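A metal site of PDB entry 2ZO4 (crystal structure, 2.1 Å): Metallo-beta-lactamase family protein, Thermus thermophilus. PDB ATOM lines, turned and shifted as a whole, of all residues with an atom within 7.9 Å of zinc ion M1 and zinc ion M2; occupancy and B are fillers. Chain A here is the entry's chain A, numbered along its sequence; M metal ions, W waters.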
ATOM      1  N   ILE A  15      34.846  23.039  12.450  1.00  0.00           N
ATOM      2  CA  ILE A  15      34.272  24.387  12.467  1.00  0.00           C
ATOM      3  C   ILE A  15      34.546  25.076  13.823  1.00  0.00           C
ATOM      4  O   ILE A  15      34.521  24.415  14.865  1.00  0.00           O
ATOM      5  CB  ILE A  15      32.752  24.401  12.125  1.00  0.00           C
ATOM      6  CG1 ILE A  15      31.961  23.478  13.068  1.00  0.00           C
ATOM      7  CG2 ILE A  15      32.533  24.035  10.669  1.00  0.00           C
ATOM      8  CD1 ILE A  15      30.444  23.669  12.999  1.00  0.00           C
ATOM      9  N   LEU A  19      29.486  23.293  17.975  1.00  0.00           N
ATOM     10  CA  LEU A  19      29.163  22.034  17.292  1.00  0.00           C
ATOM     11  C   LEU A  19      30.423  21.273  16.839  1.00  0.00           C
ATOM     12  O   LEU A  19      30.392  20.048  16.675  1.00  0.00           O
ATOM     13  CB  LEU A  19      28.224  22.278  16.103  1.00  0.00           C
ATOM     14  N   THR A  21      32.101  20.209  14.454  1.00  0.00           N
ATOM     15  CA  THR A  21      32.223  19.509  13.176  1.00  0.00           C
ATOM     16  C   THR A  21      30.926  19.611  12.371  1.00  0.00           C
ATOM     17  O   THR A  21      29.831  19.364  12.891  1.00  0.00           O
ATOM     18  CB  THR A  21      32.583  18.012  13.383  1.00  0.00           C
ATOM     19  OG1 THR A  21      33.706  17.900  14.272  1.00  0.00           O
ATOM     20  CG2 THR A  21      32.933  17.341  12.058  1.00  0.00           C
ATOM     21  N   VAL A  22      31.068  19.978  11.100  1.00  0.00           N
ATOM     22  CA  VAL A  22      29.954  19.973  10.162  1.00  0.00           C
ATOM     23  C   VAL A  22      30.097  18.794   9.204  1.00  0.00           C
ATOM     24  O   VAL A  22      31.210  18.434   8.813  1.00  0.00           O
ATOM     25  CB  VAL A  22      29.818  21.332   9.406  1.00  0.00           C
ATOM     26  CG1 VAL A  22      30.987  21.556   8.423  1.00  0.00           C
ATOM     27  CG2 VAL A  22      28.461  21.441   8.702  1.00  0.00           C
ATOM     28  N   ASN A  23      28.961  18.194   8.855  1.00  0.00           N
ATOM     29  CA  ASN A  23      28.913  17.109   7.879  1.00  0.00           C
ATOM     30  C   ASN A  23      28.499  17.597   6.496  1.00  0.00           C
ATOM     31  O   ASN A  23      27.355  18.067   6.305  1.00  0.00           O
ATOM     32  CB  ASN A  23      27.943  16.008   8.333  1.00  0.00           C
ATOM     33  CG  ASN A  23      28.384  15.335   9.612  1.00  0.00           C
ATOM     34  OD1 ASN A  23      29.572  15.167   9.860  1.00  0.00           O
ATOM     35  ND2 ASN A  23      27.414  14.960  10.442  1.00  0.00           N
ATOM     36  N   ASP A  37      26.263  21.324   1.077  1.00  0.00           N
ATOM     37  CA  ASP A  37      26.926  22.195   2.067  1.00  0.00           C
ATOM     38  C   ASP A  37      28.451  22.310   1.848  1.00  0.00           C
ATOM     39  O   ASP A  37      29.041  21.494   1.149  1.00  0.00           O
ATOM     40  CB  ASP A  37      26.537  21.811   3.500  1.00  0.00           C
ATOM     41  CG  ASP A  37      25.039  22.010   3.766  1.00  0.00           C
ATOM     42  OD1 ASP A  37      24.418  22.807   3.037  1.00  0.00           O
ATOM     43  OD2 ASP A  37      24.501  21.371   4.698  1.00  0.00           O
ATOM     44  N   THR A  69      21.685  23.438   2.292  1.00  0.00           N
ATOM     45  CA  THR A  69      20.551  23.191   3.172  1.00  0.00           C
ATOM     46  C   THR A  69      20.034  24.489   3.777  1.00  0.00           C
ATOM     47  O   THR A  69      18.825  24.700   3.865  1.00  0.00           O
ATOM     48  CB  THR A  69      20.891  22.178   4.292  1.00  0.00           C
ATOM     49  OG1 THR A  69      21.967  22.671   5.087  1.00  0.00           O
ATOM     50  CG2 THR A  69      21.264  20.813   3.691  1.00  0.00           C
ATOM     51  N   HIS A  70      20.962  25.371   4.169  1.00  0.00           N
ATOM     52  CA  HIS A  70      20.621  26.683   4.736  1.00  0.00           C
ATOM     53  C   HIS A  70      21.812  27.652   4.765  1.00  0.00           C
ATOM     54  O   HIS A  70      22.930  27.310   4.368  1.00  0.00           O
ATOM     55  CB  HIS A  70      19.981  26.529   6.124  1.00  0.00           C
ATOM     56  CG  HIS A  70      20.833  25.841   7.148  1.00  0.00           C
ATOM     57  ND1 HIS A  70      21.370  24.586   6.955  1.00  0.00           N
ATOM     58  CD2 HIS A  70      21.214  26.220   8.384  1.00  0.00           C
ATOM     59  CE1 HIS A  70      22.052  24.222   8.019  1.00  0.00           C
ATOM     60  NE2 HIS A  70      21.975  25.204   8.906  1.00  0.00           N
ATOM     61  N   HIS A  71      21.546  28.866   5.267  1.00  0.00           N
ATOM     62  CA  HIS A  71      22.468  30.001   5.201  1.00  0.00           C
ATOM     63  C   HIS A  71      23.484  30.090   6.342  1.00  0.00           C
ATOM     64  O   HIS A  71      24.326  30.994   6.336  1.00  0.00           O
ATOM     65  CB  HIS A  71      21.676  31.305   5.194  1.00  0.00           C
ATOM     66  CG  HIS A  71      21.105  31.671   6.528  1.00  0.00           C
ATOM     67  ND1 HIS A  71      19.935  31.127   7.009  1.00  0.00           N
ATOM     68  CD2 HIS A  71      21.559  32.497   7.498  1.00  0.00           C
ATOM     69  CE1 HIS A  71      19.678  31.611   8.210  1.00  0.00           C
ATOM     70  NE2 HIS A  71      20.647  32.444   8.525  1.00  0.00           N
ATOM     71  N   HIS A  72      23.376  29.218   7.339  1.00  0.00           N
ATOM     72  CA  HIS A  72      24.287  29.297   8.487  1.00  0.00           C
ATOM     73  C   HIS A  72      25.734  29.116   8.004  1.00  0.00           C
ATOM     74  O   HIS A  72      25.979  28.362   7.061  1.00  0.00           O
ATOM     75  CB  HIS A  72      23.910  28.298   9.592  1.00  0.00           C
ATOM     76  CG  HIS A  72      22.612  28.596  10.262  1.00  0.00           C
ATOM     77  ND1 HIS A  72      21.964  27.685  11.071  1.00  0.00           N
ATOM     78  CD2 HIS A  72      21.814  29.699  10.237  1.00  0.00           C
ATOM     79  CE1 HIS A  72      20.841  28.223  11.530  1.00  0.00           C
ATOM     80  NE2 HIS A  72      20.733  29.441  11.027  1.00  0.00           N
ATOM     81  N   PRO A  73      26.692  29.813   8.657  1.00  0.00           N
ATOM     82  CA  PRO A  73      28.064  29.907   8.147  1.00  0.00           C
ATOM     83  C   PRO A  73      28.747  28.559   7.928  1.00  0.00           C
ATOM     84  O   PRO A  73      29.511  28.404   6.968  1.00  0.00           O
ATOM     85  CB  PRO A  73      28.790  30.724   9.224  1.00  0.00           C
ATOM     86  CG  PRO A  73      27.924  30.624  10.444  1.00  0.00           C
ATOM     87  CD  PRO A  73      26.529  30.535   9.932  1.00  0.00           C
ATOM     88  N   ASP A  74      28.487  27.591   8.798  1.00  0.00           N
ATOM     89  CA  ASP A  74      29.068  26.246   8.700  1.00  0.00           C
ATOM     90  C   ASP A  74      28.590  25.415   7.498  1.00  0.00           C
ATOM     91  O   ASP A  74      29.156  24.359   7.204  1.00  0.00           O
ATOM     92  CB  ASP A  74      28.864  25.464  10.014  1.00  0.00           C
ATOM     93  CG  ASP A  74      27.408  25.435  10.483  1.00  0.00           C
ATOM     94  OD1 ASP A  74      26.690  26.455  10.341  1.00  0.00           O
ATOM     95  OD2 ASP A  74      26.983  24.386  11.002  1.00  0.00           O
ATOM     96  N   HIS A  75      27.566  25.891   6.803  1.00  0.00           N
ATOM     97  CA  HIS A  75      27.016  25.198   5.626  1.00  0.00           C
ATOM     98  C   HIS A  75      27.175  26.051   4.354  1.00  0.00           C
ATOM     99  O   HIS A  75      27.340  25.521   3.265  1.00  0.00           O
ATOM    100  CB  HIS A  75      25.536  24.867   5.857  1.00  0.00           C
ATOM    101  CG  HIS A  75      25.290  24.002   7.051  1.00  0.00           C
ATOM    102  ND1 HIS A  75      25.053  22.641   6.955  1.00  0.00           N
ATOM    103  CD2 HIS A  75      25.241  24.291   8.370  1.00  0.00           C
ATOM    104  CE1 HIS A  75      24.879  22.143   8.166  1.00  0.00           C
ATOM    105  NE2 HIS A  75      24.986  23.123   9.038  1.00  0.00           N
ATOM    106  N   HIS A 171      14.706  25.760  11.925  1.00  0.00           N
ATOM    107  CA  HIS A 171      16.121  25.969  12.193  1.00  0.00           C
ATOM    108  C   HIS A 171      16.651  27.151  11.376  1.00  0.00           C
ATOM    109  O   HIS A 171      17.456  27.946  11.861  1.00  0.00           O
ATOM    110  CB  HIS A 171      16.912  24.703  11.888  1.00  0.00           C
ATOM    111  CG  HIS A 171      18.380  24.854  12.123  1.00  0.00           C
ATOM    112  ND1 HIS A 171      18.940  24.861  13.379  1.00  0.00           N
ATOM    113  CD2 HIS A 171      19.410  25.012  11.250  1.00  0.00           C
ATOM    114  CE1 HIS A 171      20.244  25.014  13.284  1.00  0.00           C
ATOM    115  NE2 HIS A 171      20.557  25.099  12.001  1.00  0.00           N
ATOM    116  N   ALA A 172      16.200  27.248  10.130  1.00  0.00           N
ATOM    117  CA  ALA A 172      16.403  28.429   9.293  1.00  0.00           C
ATOM    118  C   ALA A 172      15.182  28.583   8.413  1.00  0.00           C
ATOM    119  O   ALA A 172      14.484  27.613   8.147  1.00  0.00           O
ATOM    120  CB  ALA A 172      17.676  28.297   8.443  1.00  0.00           C
ATOM    121  N   HIS A 175      15.355  26.646   5.165  1.00  0.00           N
ATOM    122  CA  HIS A 175      16.074  25.397   5.340  1.00  0.00           C
ATOM    123  C   HIS A 175      15.452  24.342   4.427  1.00  0.00           C
ATOM    124  O   HIS A 175      14.231  24.181   4.372  1.00  0.00           O
ATOM    125  CB  HIS A 175      16.082  24.936   6.787  1.00  0.00           C
ATOM    126  CG  HIS A 175      16.922  23.726   7.020  1.00  0.00           C
ATOM    127  ND1 HIS A 175      16.481  22.446   6.766  1.00  0.00           N
ATOM    128  CD2 HIS A 175      18.203  23.593   7.456  1.00  0.00           C
ATOM    129  CE1 HIS A 175      17.445  21.587   7.044  1.00  0.00           C
ATOM    130  NE2 HIS A 175      18.489  22.258   7.463  1.00  0.00           N
ATOM    131  N   GLY A 189      20.199  18.004   6.642  1.00  0.00           N
ATOM    132  CA  GLY A 189      20.779  19.281   7.073  1.00  0.00           C
ATOM    133  C   GLY A 189      20.681  19.398   8.590  1.00  0.00           C
ATOM    134  O   GLY A 189      20.959  18.440   9.294  1.00  0.00           O
ATOM    135  N   ASP A 190      20.270  20.562   9.077  1.00  0.00           N
ATOM    136  CA  ASP A 190      20.054  20.738  10.506  1.00  0.00           C
ATOM    137  C   ASP A 190      18.583  20.739  10.920  1.00  0.00           C
ATOM    138  O   ASP A 190      18.229  21.274  11.963  1.00  0.00           O
ATOM    139  CB  ASP A 190      20.733  22.022  11.011  1.00  0.00           C
ATOM    140  CG  ASP A 190      22.254  21.977  10.897  1.00  0.00           C
ATOM    141  OD1 ASP A 190      22.816  20.953  10.434  1.00  0.00           O
ATOM    142  OD2 ASP A 190      22.882  22.981  11.272  1.00  0.00           O
ATOM    143  N   ALA A 191      17.708  20.148  10.100  1.00  0.00           N
ATOM    144  CA  ALA A 191      16.286  20.026  10.450  1.00  0.00           C
ATOM    145  C   ALA A 191      16.085  18.954  11.520  1.00  0.00           C
ATOM    146  O   ALA A 191      15.067  18.931  12.218  1.00  0.00           O
ATOM    147  CB  ALA A 191      15.460  19.704   9.200  1.00  0.00           C
ATOM    148  N   LEU A 193      18.743  16.353  14.185  1.00  0.00           N
ATOM    149  CA  LEU A 193      20.052  15.895  14.686  1.00  0.00           C
ATOM    150  C   LEU A 193      19.833  14.793  15.716  1.00  0.00           C
ATOM    151  O   LEU A 193      18.798  14.774  16.381  1.00  0.00           O
ATOM    152  CB  LEU A 193      20.834  17.049  15.316  1.00  0.00           C
ATOM    153  CG  LEU A 193      21.278  18.259  14.474  1.00  0.00           C
ATOM    154  CD1 LEU A 193      21.881  19.331  15.360  1.00  0.00           C
ATOM    155  CD2 LEU A 193      22.246  17.856  13.372  1.00  0.00           C
ATOM    156  N   PRO A 198      18.728  20.760  17.052  1.00  0.00           N
ATOM    157  CA  PRO A 198      19.243  21.891  16.298  1.00  0.00           C
ATOM    158  C   PRO A 198      18.603  23.182  16.808  1.00  0.00           C
ATOM    159  O   PRO A 198      17.450  23.169  17.256  1.00  0.00           O
ATOM    160  CB  PRO A 198      18.804  21.602  14.856  1.00  0.00           C
ATOM    161  CG  PRO A 198      17.742  20.564  14.960  1.00  0.00           C
ATOM    162  CD  PRO A 198      18.050  19.768  16.180  1.00  0.00           C
ATOM    163  N   ASN A 199      19.355  24.273  16.761  1.00  0.00           N
ATOM    164  CA  ASN A 199      18.861  25.583  17.158  1.00  0.00           C
ATOM    165  C   ASN A 199      17.530  25.913  16.483  1.00  0.00           C
ATOM    166  O   ASN A 199      17.318  25.592  15.303  1.00  0.00           O
ATOM    167  CB  ASN A 199      19.894  26.662  16.823  1.00  0.00           C
ATOM    168  CG  ASN A 199      19.811  27.872  17.734  1.00  0.00           C
ATOM    169  OD1 ASN A 199      20.070  27.785  18.941  1.00  0.00           O
ATOM    170  ND2 ASN A 199      19.458  29.029  17.167  1.00  0.00           N
ATOM    171  N   ALA A 231      22.627  13.893   8.740  1.00  0.00           N
ATOM    172  CA  ALA A 231      22.378  15.281   9.089  1.00  0.00           C
ATOM    173  C   ALA A 231      23.645  16.142   9.022  1.00  0.00           C
ATOM    174  O   ALA A 231      24.722  15.638   8.693  1.00  0.00           O
ATOM    175  CB  ALA A 231      21.740  15.363  10.464  1.00  0.00           C
ATOM    176  N   GLY A 232      23.501  17.422   9.334  1.00  0.00           N
ATOM    177  CA  GLY A 232      24.597  18.383   9.256  1.00  0.00           C
ATOM    178  C   GLY A 232      25.612  18.255  10.366  1.00  0.00           C
ATOM    179  O   GLY A 232      26.748  18.717  10.236  1.00  0.00           O
ATOM    180  N   HIS A 233      25.205  17.624  11.468  1.00  0.00           N
ATOM    181  CA  HIS A 233      26.107  17.393  12.599  1.00  0.00           C
ATOM    182  C   HIS A 233      25.830  16.036  13.239  1.00  0.00           C
ATOM    183  O   HIS A 233      24.738  15.479  13.089  1.00  0.00           O
ATOM    184  CB  HIS A 233      25.958  18.504  13.645  1.00  0.00           C
ATOM    185  CG  HIS A 233      26.118  19.879  13.090  1.00  0.00           C
ATOM    186  ND1 HIS A 233      27.342  20.455  12.852  1.00  0.00           N
ATOM    187  CD2 HIS A 233      25.188  20.792  12.708  1.00  0.00           C
ATOM    188  CE1 HIS A 233      27.177  21.667  12.351  1.00  0.00           C
ATOM    189  NE2 HIS A 233      25.880  21.895  12.253  1.00  0.00           N
ATOM    190  N   PHE A 287      23.105  31.951  20.712  1.00  0.00           N
ATOM    191  CA  PHE A 287      22.165  30.924  20.262  1.00  0.00           C
ATOM    192  C   PHE A 287      21.147  30.579  21.341  1.00  0.00           C
ATOM    193  O   PHE A 287      19.973  30.372  21.057  1.00  0.00           O
ATOM    194  CB  PHE A 287      22.906  29.665  19.804  1.00  0.00           C
ATOM    195  CG  PHE A 287      23.894  29.920  18.695  1.00  0.00           C
ATOM    196  CD1 PHE A 287      25.261  29.746  18.916  1.00  0.00           C
ATOM    197  CD2 PHE A 287      23.466  30.345  17.439  1.00  0.00           C
ATOM    198  CE1 PHE A 287      26.180  29.987  17.900  1.00  0.00           C
ATOM    199  CE2 PHE A 287      24.388  30.596  16.421  1.00  0.00           C
ATOM    200  CZ  PHE A 287      25.752  30.412  16.645  1.00  0.00           C
HETATM  201 ZN    ZN M   1      22.384  25.496  11.087  1.00  0.00          ZN
HETATM  202 ZN    ZN M   2      24.905  23.357  11.085  1.00  0.00          ZN
HETATM  203  O   HOH W   1      24.318  25.192  11.535  1.00  0.00           O
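The side-chain carboxylate (OD2) of Asp 37 lies within hydrogen-bond range of a ring nitrogen (ND1) of His 75, at 2.6 Å. A ring nitrogen (NE2) of His 175 sits at hydrogen-bond distance from the backbone NH (N) of Asp 190, 2.9 Å away. A ring nitrogen (ND1) of His 171 lies within hydrogen-bond range of the backbone carbonyl oxygen (O) of Asn 199 (2.6 Å). The backbone carbonyl oxygen of Thr 21 sits at hydrogen-bond distance from a ring nitrogen (ND1) of His 233, at 2.7 Å. A ring nitrogen (ND1) of His 70 sits at hydrogen-bond distance from the side-chain hydroxyl (OG1) of Thr 69 (2.7 Å).
Zinc ion M2 is bound by water W1 (2.0 Å), a ring nitrogen (NE2) of His 75 (2.1 Å), the side-chain carboxylate of Asp 190 (2.1 Å), a ring nitrogen (NE2) of His 233 (2.1 Å) and the side-chain carboxylate of Asp 74 (2.3 Å).
Four residues have an atom within 4 Å of zinc ion M1: His 70, His 72, His 171 and Asp 190. Along chain A the residues within 4 Å of zinc ion M1 span positions 70 to 190.
Zinc ion M1 is bound by water W1, at 2.0 Å. NE2 of His 171 binds zinc ion M1, 2.1 Å away. ND1 of His 72 binds zinc ion M1, 2.2 Å away. Zinc ion M1 is bound by NE2 of His 70 (2.2 Å). Zinc ion M1 is bound by OD2 of Asp 190, 2.6 Å away.
Four residues have an atom within 4 Å of zinc ion M2: Asp 74, His 75, Asp 190 and His 233. Along chain A the residues within 4 Å of zinc ion M2 span positions 74 to 233.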
